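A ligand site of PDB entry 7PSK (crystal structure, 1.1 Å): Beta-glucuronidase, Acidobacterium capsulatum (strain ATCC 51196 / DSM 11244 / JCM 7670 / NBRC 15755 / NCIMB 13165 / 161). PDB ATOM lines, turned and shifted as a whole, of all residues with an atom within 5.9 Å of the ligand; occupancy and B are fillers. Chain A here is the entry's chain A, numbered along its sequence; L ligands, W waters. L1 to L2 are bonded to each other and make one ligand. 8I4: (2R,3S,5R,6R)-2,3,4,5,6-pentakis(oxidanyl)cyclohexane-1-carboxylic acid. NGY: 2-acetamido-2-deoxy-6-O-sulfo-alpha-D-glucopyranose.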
ATOM      1  N   GLU A  45      16.473 -22.863  29.778  1.00  0.00           N
ATOM      2  CA  GLU A  45      16.354 -22.875  28.316  1.00  0.00           C
ATOM      3  C   GLU A  45      14.908 -22.604  27.895  1.00  0.00           C
ATOM      4  O   GLU A  45      13.975 -23.171  28.438  1.00  0.00           O
ATOM      5  CB  GLU A  45      16.730 -24.251  27.820  1.00  0.00           C
ATOM      6  CG  GLU A  45      18.195 -24.522  27.976  1.00  0.00           C
ATOM      7  CD  GLU A  45      19.097 -23.641  27.172  1.00  0.00           C
ATOM      8  OE1 GLU A  45      18.693 -23.079  26.119  1.00  0.00           O
ATOM      9  OE2 GLU A  45      20.259 -23.463  27.602  1.00  0.00           O
ATOM     10  N   ARG A  76      14.752 -16.222  34.296  1.00  0.00           N
ATOM     11  CA  ARG A  76      15.184 -15.882  32.933  1.00  0.00           C
ATOM     12  C   ARG A  76      15.029 -17.139  32.093  1.00  0.00           C
ATOM     13  O   ARG A  76      15.544 -18.187  32.467  1.00  0.00           O
ATOM     14  CB  ARG A  76      16.606 -15.340  32.913  1.00  0.00           C
ATOM     15  CG  ARG A  76      17.109 -15.010  31.514  1.00  0.00           C
ATOM     16  CD  ARG A  76      17.962 -16.118  30.968  1.00  0.00           C
ATOM     17  NE  ARG A  76      18.422 -15.811  29.611  1.00  0.00           N
ATOM     18  CZ  ARG A  76      19.456 -16.414  29.041  1.00  0.00           C
ATOM     19  NH1 ARG A  76      20.105 -17.363  29.655  1.00  0.00           N
ATOM     20  NH2 ARG A  76      19.808 -16.068  27.803  1.00  0.00           N
ATOM     21  N   GLY A  78      15.771 -18.380  28.176  1.00  0.00           N
ATOM     22  CA  GLY A  78      16.444 -17.997  26.943  1.00  0.00           C
ATOM     23  C   GLY A  78      17.414 -19.069  26.544  1.00  0.00           C
ATOM     24  O   GLY A  78      16.999 -20.212  26.265  1.00  0.00           O
ATOM     25  N   GLY A  79      18.689 -18.762  26.494  1.00  0.00           N
ATOM     26  CA  GLY A  79      19.693 -19.780  26.219  1.00  0.00           C
ATOM     27  C   GLY A  79      19.784 -20.095  24.747  1.00  0.00           C
ATOM     28  O   GLY A  79      19.078 -19.557  23.893  1.00  0.00           O
ATOM     29  N   ASN A  80      20.688 -20.972  24.452  1.00  0.00           N
ATOM     30  CA  ASN A  80      20.940 -21.366  23.046  1.00  0.00           C
ATOM     31  C   ASN A  80      19.704 -21.980  22.440  1.00  0.00           C
ATOM     32  O   ASN A  80      19.566 -21.905  21.195  1.00  0.00           O
ATOM     33  CB  ASN A  80      22.075 -22.392  22.967  1.00  0.00           C
ATOM     34  CG  ASN A  80      23.395 -21.909  23.364  1.00  0.00           C
ATOM     35  OD1 ASN A  80      23.605 -20.712  23.540  1.00  0.00           O
ATOM     36  ND2 ASN A  80      24.290 -22.852  23.486  1.00  0.00           N
ATOM     37  N   THR A  81      18.843 -22.588  23.221  1.00  0.00           N
ATOM     38  CA  THR A  81      17.662 -23.198  22.584  1.00  0.00           C
ATOM     39  C   THR A  81      16.715 -22.127  22.055  1.00  0.00           C
ATOM     40  O   THR A  81      15.801 -22.503  21.265  1.00  0.00           O
ATOM     41  CB  THR A  81      16.930 -24.125  23.527  1.00  0.00           C
ATOM     42  OG1 THR A  81      16.439 -23.423  24.660  1.00  0.00           O
ATOM     43  CG2 THR A  81      17.773 -25.302  23.928  1.00  0.00           C
ATOM     44  N   GLU A  83      17.450 -20.244  19.866  1.00  0.00           N
ATOM     45  CA  GLU A  83      17.740 -20.247  18.406  1.00  0.00           C
ATOM     46  C   GLU A  83      16.679 -21.025  17.680  1.00  0.00           C
ATOM     47  O   GLU A  83      16.449 -20.745  16.488  1.00  0.00           O
ATOM     48  CB  GLU A  83      19.079 -20.968  18.154  1.00  0.00           C
ATOM     49  CG  GLU A  83      20.248 -20.146  18.675  1.00  0.00           C
ATOM     50  CD  GLU A  83      21.543 -20.921  18.834  1.00  0.00           C
ATOM     51  OE1 GLU A  83      21.688 -22.078  18.280  1.00  0.00           O
ATOM     52  OE2 GLU A  83      22.420 -20.385  19.534  1.00  0.00           O
ATOM     53  N   ASN A 172      20.082 -14.766  22.400  1.00  0.00           N
ATOM     54  CA  ASN A 172      21.042 -15.146  23.419  1.00  0.00           C
ATOM     55  C   ASN A 172      22.414 -15.220  22.827  1.00  0.00           C
ATOM     56  O   ASN A 172      22.605 -15.833  21.755  1.00  0.00           O
ATOM     57  CB  ASN A 172      20.591 -16.508  23.968  1.00  0.00           C
ATOM     58  CG  ASN A 172      21.644 -17.167  24.817  1.00  0.00           C
ATOM     59  OD1 ASN A 172      21.844 -16.860  25.993  1.00  0.00           O
ATOM     60  ND2 ASN A 172      22.358 -18.142  24.232  1.00  0.00           N
ATOM     61  N   GLU A 173      23.379 -14.605  23.469  1.00  0.00           N
ATOM     62  CA  GLU A 173      24.801 -14.695  23.044  1.00  0.00           C
ATOM     63  C   GLU A 173      24.924 -14.523  21.535  1.00  0.00           C
ATOM     64  O   GLU A 173      25.476 -15.365  20.834  1.00  0.00           O
ATOM     65  CB  GLU A 173      25.398 -15.984  23.505  1.00  0.00           C
ATOM     66  CG  GLU A 173      25.385 -16.078  25.030  1.00  0.00           C
ATOM     67  CD  GLU A 173      26.257 -17.107  25.692  1.00  0.00           C
ATOM     68  OE1 GLU A 173      26.640 -18.053  25.030  1.00  0.00           O
ATOM     69  OE2 GLU A 173      26.509 -16.957  26.918  1.00  0.00           O
ATOM     70  N   ASN A 180      27.842 -21.920  15.396  1.00  0.00           N
ATOM     71  CA  ASN A 180      27.044 -23.032  14.841  1.00  0.00           C
ATOM     72  C   ASN A 180      26.264 -22.561  13.608  1.00  0.00           C
ATOM     73  O   ASN A 180      25.315 -23.248  13.248  1.00  0.00           O
ATOM     74  CB  ASN A 180      26.136 -23.660  15.890  1.00  0.00           C
ATOM     75  CG  ASN A 180      25.103 -22.678  16.373  1.00  0.00           C
ATOM     76  OD1 ASN A 180      25.218 -21.472  16.116  1.00  0.00           O
ATOM     77  ND2 ASN A 180      24.131 -23.186  17.118  1.00  0.00           N
ATOM     78  N   HIS A 241      26.556 -12.220  30.804  1.00  0.00           N
ATOM     79  CA  HIS A 241      26.733 -13.620  31.181  1.00  0.00           C
ATOM     80  C   HIS A 241      28.104 -13.810  31.773  1.00  0.00           C
ATOM     81  O   HIS A 241      29.042 -13.002  31.499  1.00  0.00           O
ATOM     82  CB  HIS A 241      26.612 -14.549  29.999  1.00  0.00           C
ATOM     83  CG  HIS A 241      25.253 -14.518  29.397  1.00  0.00           C
ATOM     84  ND1 HIS A 241      24.949 -15.314  28.339  1.00  0.00           N
ATOM     85  CD2 HIS A 241      24.132 -13.832  29.723  1.00  0.00           C
ATOM     86  CE1 HIS A 241      23.649 -15.105  28.069  1.00  0.00           C
ATOM     87  NE2 HIS A 241      23.144 -14.272  28.830  1.00  0.00           N
ATOM     88  N   TYR A 243      30.710 -17.298  32.937  1.00  0.00           N
ATOM     89  CA  TYR A 243      31.103 -18.658  33.383  1.00  0.00           C
ATOM     90  C   TYR A 243      32.523 -18.597  33.955  1.00  0.00           C
ATOM     91  O   TYR A 243      33.398 -18.019  33.254  1.00  0.00           O
ATOM     92  CB  TYR A 243      30.979 -19.642  32.225  1.00  0.00           C
ATOM     93  CG  TYR A 243      29.544 -20.051  31.977  1.00  0.00           C
ATOM     94  CD1 TYR A 243      28.652 -19.177  31.407  1.00  0.00           C
ATOM     95  CD2 TYR A 243      29.065 -21.270  32.424  1.00  0.00           C
ATOM     96  CE1 TYR A 243      27.343 -19.533  31.173  1.00  0.00           C
ATOM     97  CE2 TYR A 243      27.748 -21.627  32.237  1.00  0.00           C
ATOM     98  CZ  TYR A 243      26.877 -20.752  31.623  1.00  0.00           C
ATOM     99  OH  TYR A 243      25.582 -21.162  31.440  1.00  0.00           O
ATOM    100  N   GLU A 287      22.901 -15.044  32.875  1.00  0.00           N
ATOM    101  CA  GLU A 287      23.211 -16.465  32.710  1.00  0.00           C
ATOM    102  C   GLU A 287      24.595 -16.664  33.308  1.00  0.00           C
ATOM    103  O   GLU A 287      25.566 -16.037  32.831  1.00  0.00           O
ATOM    104  CB  GLU A 287      23.237 -16.881  31.248  1.00  0.00           C
ATOM    105  CG  GLU A 287      23.356 -18.381  31.076  1.00  0.00           C
ATOM    106  CD  GLU A 287      23.515 -18.764  29.632  1.00  0.00           C
ATOM    107  OE1 GLU A 287      23.086 -18.072  28.743  1.00  0.00           O
ATOM    108  OE2 GLU A 287      24.160 -19.830  29.399  1.00  0.00           O
ATOM    109  N   CYS A 291      30.954 -23.691  35.062  1.00  0.00           N
ATOM    110  CA  CYS A 291      31.550 -24.167  33.838  1.00  0.00           C
ATOM    111  C   CYS A 291      30.482 -24.148  32.783  1.00  0.00           C
ATOM    112  O   CYS A 291      29.296 -24.416  33.053  1.00  0.00           O
ATOM    113  CB  CYS A 291      32.072 -25.581  34.010  1.00  0.00           C
ATOM    114  SG  CYS A 291      33.423 -25.724  35.192  1.00  0.00           S
ATOM    115  N   TYR A 292      30.854 -23.916  31.562  1.00  0.00           N
ATOM    116  CA  TYR A 292      29.896 -23.906  30.453  1.00  0.00           C
ATOM    117  C   TYR A 292      29.841 -25.315  29.874  1.00  0.00           C
ATOM    118  O   TYR A 292      30.252 -26.347  30.466  1.00  0.00           O
ATOM    119  CB  TYR A 292      30.177 -22.769  29.477  1.00  0.00           C
ATOM    120  CG  TYR A 292      31.590 -22.764  28.968  1.00  0.00           C
ATOM    121  CD1 TYR A 292      32.062 -23.635  27.996  1.00  0.00           C
ATOM    122  CD2 TYR A 292      32.505 -21.866  29.454  1.00  0.00           C
ATOM    123  CE1 TYR A 292      33.399 -23.654  27.594  1.00  0.00           C
ATOM    124  CE2 TYR A 292      33.851 -21.840  29.080  1.00  0.00           C
ATOM    125  CZ  TYR A 292      34.303 -22.769  28.147  1.00  0.00           C
ATOM    126  OH  TYR A 292      35.606 -22.840  27.699  1.00  0.00           O
ATOM    127  N   GLN A 293      29.162 -25.377  28.740  1.00  0.00           N
ATOM    128  CA  GLN A 293      28.785 -26.650  28.102  1.00  0.00           C
ATOM    129  C   GLN A 293      28.210 -27.635  29.133  1.00  0.00           C
ATOM    130  O   GLN A 293      28.624 -28.774  29.119  1.00  0.00           O
ATOM    131  CB  GLN A 293      30.004 -27.177  27.334  1.00  0.00           C
ATOM    132  N   GLY A 294      27.252 -27.166  29.977  1.00  0.00           N
ATOM    133  CA  GLY A 294      26.438 -27.964  30.877  1.00  0.00           C
ATOM    134  C   GLY A 294      27.101 -28.234  32.224  1.00  0.00           C
ATOM    135  O   GLY A 294      26.466 -28.829  33.065  1.00  0.00           O
ATOM    136  N   GLY A 295      28.302 -27.733  32.402  1.00  0.00           N
ATOM    137  CA  GLY A 295      29.002 -27.971  33.654  1.00  0.00           C
ATOM    138  C   GLY A 295      29.992 -29.087  33.549  1.00  0.00           C
ATOM    139  O   GLY A 295      29.932 -29.879  32.607  1.00  0.00           O
ATOM    140  N   HIS A 327      22.241 -20.704  35.512  1.00  0.00           N
ATOM    141  CA  HIS A 327      21.663 -21.534  34.465  1.00  0.00           C
ATOM    142  C   HIS A 327      21.507 -22.957  34.893  1.00  0.00           C
ATOM    143  O   HIS A 327      22.325 -23.506  35.639  1.00  0.00           O
ATOM    144  CB  HIS A 327      22.526 -21.448  33.207  1.00  0.00           C
ATOM    145  CG  HIS A 327      21.796 -21.784  31.944  1.00  0.00           C
ATOM    146  ND1 HIS A 327      20.727 -21.037  31.533  1.00  0.00           N
ATOM    147  CD2 HIS A 327      21.961 -22.819  31.101  1.00  0.00           C
ATOM    148  CE1 HIS A 327      20.304 -21.636  30.434  1.00  0.00           C
ATOM    149  NE2 HIS A 327      20.993 -22.670  30.155  1.00  0.00           N
ATOM    150  N   GLY A 328      20.501 -23.610  34.404  1.00  0.00           N
ATOM    151  CA  GLY A 328      20.199 -24.973  34.800  1.00  0.00           C
ATOM    152  C   GLY A 328      19.014 -25.518  34.061  1.00  0.00           C
ATOM    153  O   GLY A 328      18.568 -24.946  33.074  1.00  0.00           O
ATOM    154  N   GLY A 329      18.554 -26.639  34.584  1.00  0.00           N
ATOM    155  CA  GLY A 329      17.486 -27.449  33.982  1.00  0.00           C
ATOM    156  C   GLY A 329      17.936 -28.857  33.838  1.00  0.00           C
ATOM    157  O   GLY A 329      19.113 -29.241  33.849  1.00  0.00           O
ATOM    158  N   GLY A 330      16.967 -29.750  33.773  1.00  0.00           N
ATOM    159  CA  GLY A 330      17.231 -31.184  33.622  1.00  0.00           C
ATOM    160  C   GLY A 330      18.012 -31.723  34.776  1.00  0.00           C
ATOM    161  O   GLY A 330      17.716 -31.440  35.955  1.00  0.00           O
ATOM    162  N   TYR A 334      25.651 -28.612  36.302  1.00  0.00           N
ATOM    163  CA  TYR A 334      25.659 -27.348  37.040  1.00  0.00           C
ATOM    164  C   TYR A 334      24.285 -26.923  37.557  1.00  0.00           C
ATOM    165  O   TYR A 334      24.189 -25.847  38.134  1.00  0.00           O
ATOM    166  CB  TYR A 334      26.297 -26.237  36.200  1.00  0.00           C
ATOM    167  CG  TYR A 334      25.697 -25.903  34.859  1.00  0.00           C
ATOM    168  CD1 TYR A 334      24.353 -26.095  34.520  1.00  0.00           C
ATOM    169  CD2 TYR A 334      26.539 -25.360  33.907  1.00  0.00           C
ATOM    170  CE1 TYR A 334      23.906 -25.770  33.252  1.00  0.00           C
ATOM    171  CE2 TYR A 334      26.081 -24.984  32.653  1.00  0.00           C
ATOM    172  CZ  TYR A 334      24.780 -25.250  32.325  1.00  0.00           C
ATOM    173  OH  TYR A 334      24.295 -24.992  31.072  1.00  0.00           O
HETATM  174  C3  8I4 L   1      23.179 -21.981  27.384  1.00  0.00           C
HETATM  175  C5  8I4 L   1      25.298 -22.580  28.533  1.00  0.00           C
HETATM  176  C6  8I4 L   1      26.336 -23.602  28.670  1.00  0.00           C
HETATM  177  O3  8I4 L   1      22.219 -22.358  26.366  1.00  0.00           O
HETATM  178  O4  8I4 L   1      23.784 -24.279  27.994  1.00  0.00           O
HETATM  179  C1  8I4 L   1      24.741 -20.144  28.042  1.00  0.00           C
HETATM  180  C2  8I4 L   1      23.808 -20.673  26.933  1.00  0.00           C
HETATM  181  C4  8I4 L   1      24.272 -23.007  27.494  1.00  0.00           C
HETATM  182  C7  8I4 L   1      25.855 -21.189  28.235  1.00  0.00           C
HETATM  183  O2  8I4 L   1      22.852 -19.702  26.622  1.00  0.00           O
HETATM  184  O6B 8I4 L   1      26.315 -24.435  29.602  1.00  0.00           O
HETATM  185  O6A 8I4 L   1      27.255 -23.674  27.802  1.00  0.00           O
HETATM  186  O7  8I4 L   1      26.580 -21.242  26.967  1.00  0.00           O
HETATM  187  C1  NGY L   2      23.126 -25.139  27.113  1.00  0.00           C
HETATM  188  C2  NGY L   2      22.841 -26.418  27.845  1.00  0.00           C
HETATM  189  C3  NGY L   2      24.089 -27.232  28.107  1.00  0.00           C
HETATM  190  C4  NGY L   2      24.774 -27.475  26.801  1.00  0.00           C
HETATM  191  C5  NGY L   2      25.052 -26.134  26.181  1.00  0.00           C
HETATM  192  C6  NGY L   2      25.699 -26.273  24.835  1.00  0.00           C
HETATM  193  O3  NGY L   2      23.708 -28.484  28.691  1.00  0.00           O
HETATM  194  O4  NGY L   2      26.022 -28.159  27.011  1.00  0.00           O
HETATM  195  O5  NGY L   2      23.849 -25.396  25.954  1.00  0.00           O
HETATM  196  O6  NGY L   2      24.901 -27.013  23.959  1.00  0.00           O
HETATM  197  N2  NGY L   2      22.228 -26.128  29.144  1.00  0.00           N
HETATM  198  C7  NGY L   2      21.005 -26.519  29.480  1.00  0.00           C
HETATM  199  O7  NGY L   2      20.268 -27.135  28.692  1.00  0.00           O
HETATM  200  C8  NGY L   2      20.533 -26.205  30.873  1.00  0.00           C
HETATM  201  S   NGY L   2      24.929 -26.764  22.412  1.00  0.00           S
HETATM  202  O7A NGY L   2      24.373 -25.437  22.116  1.00  0.00           O
HETATM  203  O8  NGY L   2      26.316 -26.785  22.013  1.00  0.00           O
HETATM  204  O9  NGY L   2      24.121 -27.862  21.912  1.00  0.00           O
HETATM  205  O   HOH W   1      25.358 -30.885  28.258  1.00  0.00           O
HETATM  206  O   HOH W   2      28.594 -19.531  26.157  1.00  0.00           O
HETATM  207  O   HOH W   3      17.651 -27.466  29.536  1.00  0.00           O
HETATM  208  O   HOH W   4      21.540 -27.939  33.629  1.00  0.00           O
HETATM  209  O   HOH W   5      22.668 -29.053  31.149  1.00  0.00           O
HETATM  210  O   HOH W   6      21.440 -26.270  24.220  1.00  0.00           O
HETATM  211  O   HOH W   7      19.865 -27.479  26.011  1.00  0.00           O
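The side-chain amide nitrogen (ND2) of Asn 172 lies within hydrogen-bond range of an oxygen (O2) of 8I4 L1 (2.9 Å).
The side-chain amide nitrogen (ND2) of Asn 80 lies within hydrogen-bond range of an oxygen (O7A) of NGY L2.
The backbone NH of Gly 294 lies within hydrogen-bond range of an oxygen (O6B) of 8I4 L1, 2.9 Å away.
The side-chain hydroxyl (OH) of Tyr 334 lies within hydrogen-bond range of an oxygen (O6B) of 8I4 L1.
The side-chain carboxylate of Glu 45 is in hydrogen-bond range of an oxygen (O3) of 8I4 L1, at 2.6 Å.
The side-chain carboxylate of Glu 287 is covalently linked to a carbon (C1) of 8I4 L1 (1.5 Å).
O of Gln 293 lies close to O4 of NGY L2, at 3.4 Å.
The backbone NH (N) of Asn 80 lies within hydrogen-bond range of an oxygen (O3) of 8I4 L1.
The backbone NH (N) of Gln 293 sits at hydrogen-bond distance from an oxygen (O6A) of 8I4 L1 (2.7 Å).
OD1 of Asn 172 lies close to OE1 of Glu 287, 3.3 Å away.
The side-chain amide oxygen (OD1) of Asn 172 lies within hydrogen-bond range of the guanidinium group (NH2) of Arg 76, 2.8 Å away.
The side-chain amide nitrogen (ND2) of Asn 172 is in hydrogen-bond range of the side-chain amide oxygen (OD1) of Asn 80, 2.9 Å away.
The side-chain carboxylate of Glu 287 lies close to a ring nitrogen (ND1) of His 241, at 3.4 Å.
The side-chain carboxylate (OE1) of Glu 45 is in hydrogen-bond range of the backbone NH (N) of Asn 80.
The side-chain carboxylate (OE2) of Glu 287 is in hydrogen-bond range of the side-chain hydroxyl (OH) of Tyr 243, 2.8 Å away.
The side-chain carboxylate of Glu 45 is in hydrogen-bond range of the side-chain hydroxyl of Thr 81, at 2.7 Å.
The side-chain carboxylate (OE1) of Glu 287 lies within salt-bridge range of the guanidinium group (NH1) of Arg 76.
Gly 79 touches the ligand.
Glu 173 touches the ligand.
OH of Tyr 243 touches C7 of 8I4 L1 (3.2 Å).
CB of Tyr 292 touches O6A of 8I4 L1 (3.5 Å).
NE2 of His 327 touches C3 of 8I4 L1, at 3.6 Å.
Gly 328 touches the ligand.
Hydrophobic or aromatic side chains within 4 Å of the ligand: Tyr 243, Tyr 292, His 327 and Tyr 334.
Water W2 bridges OE1 of Glu 173 (2.7 Å) and O7 of 8I4 L1 (2.8 Å).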
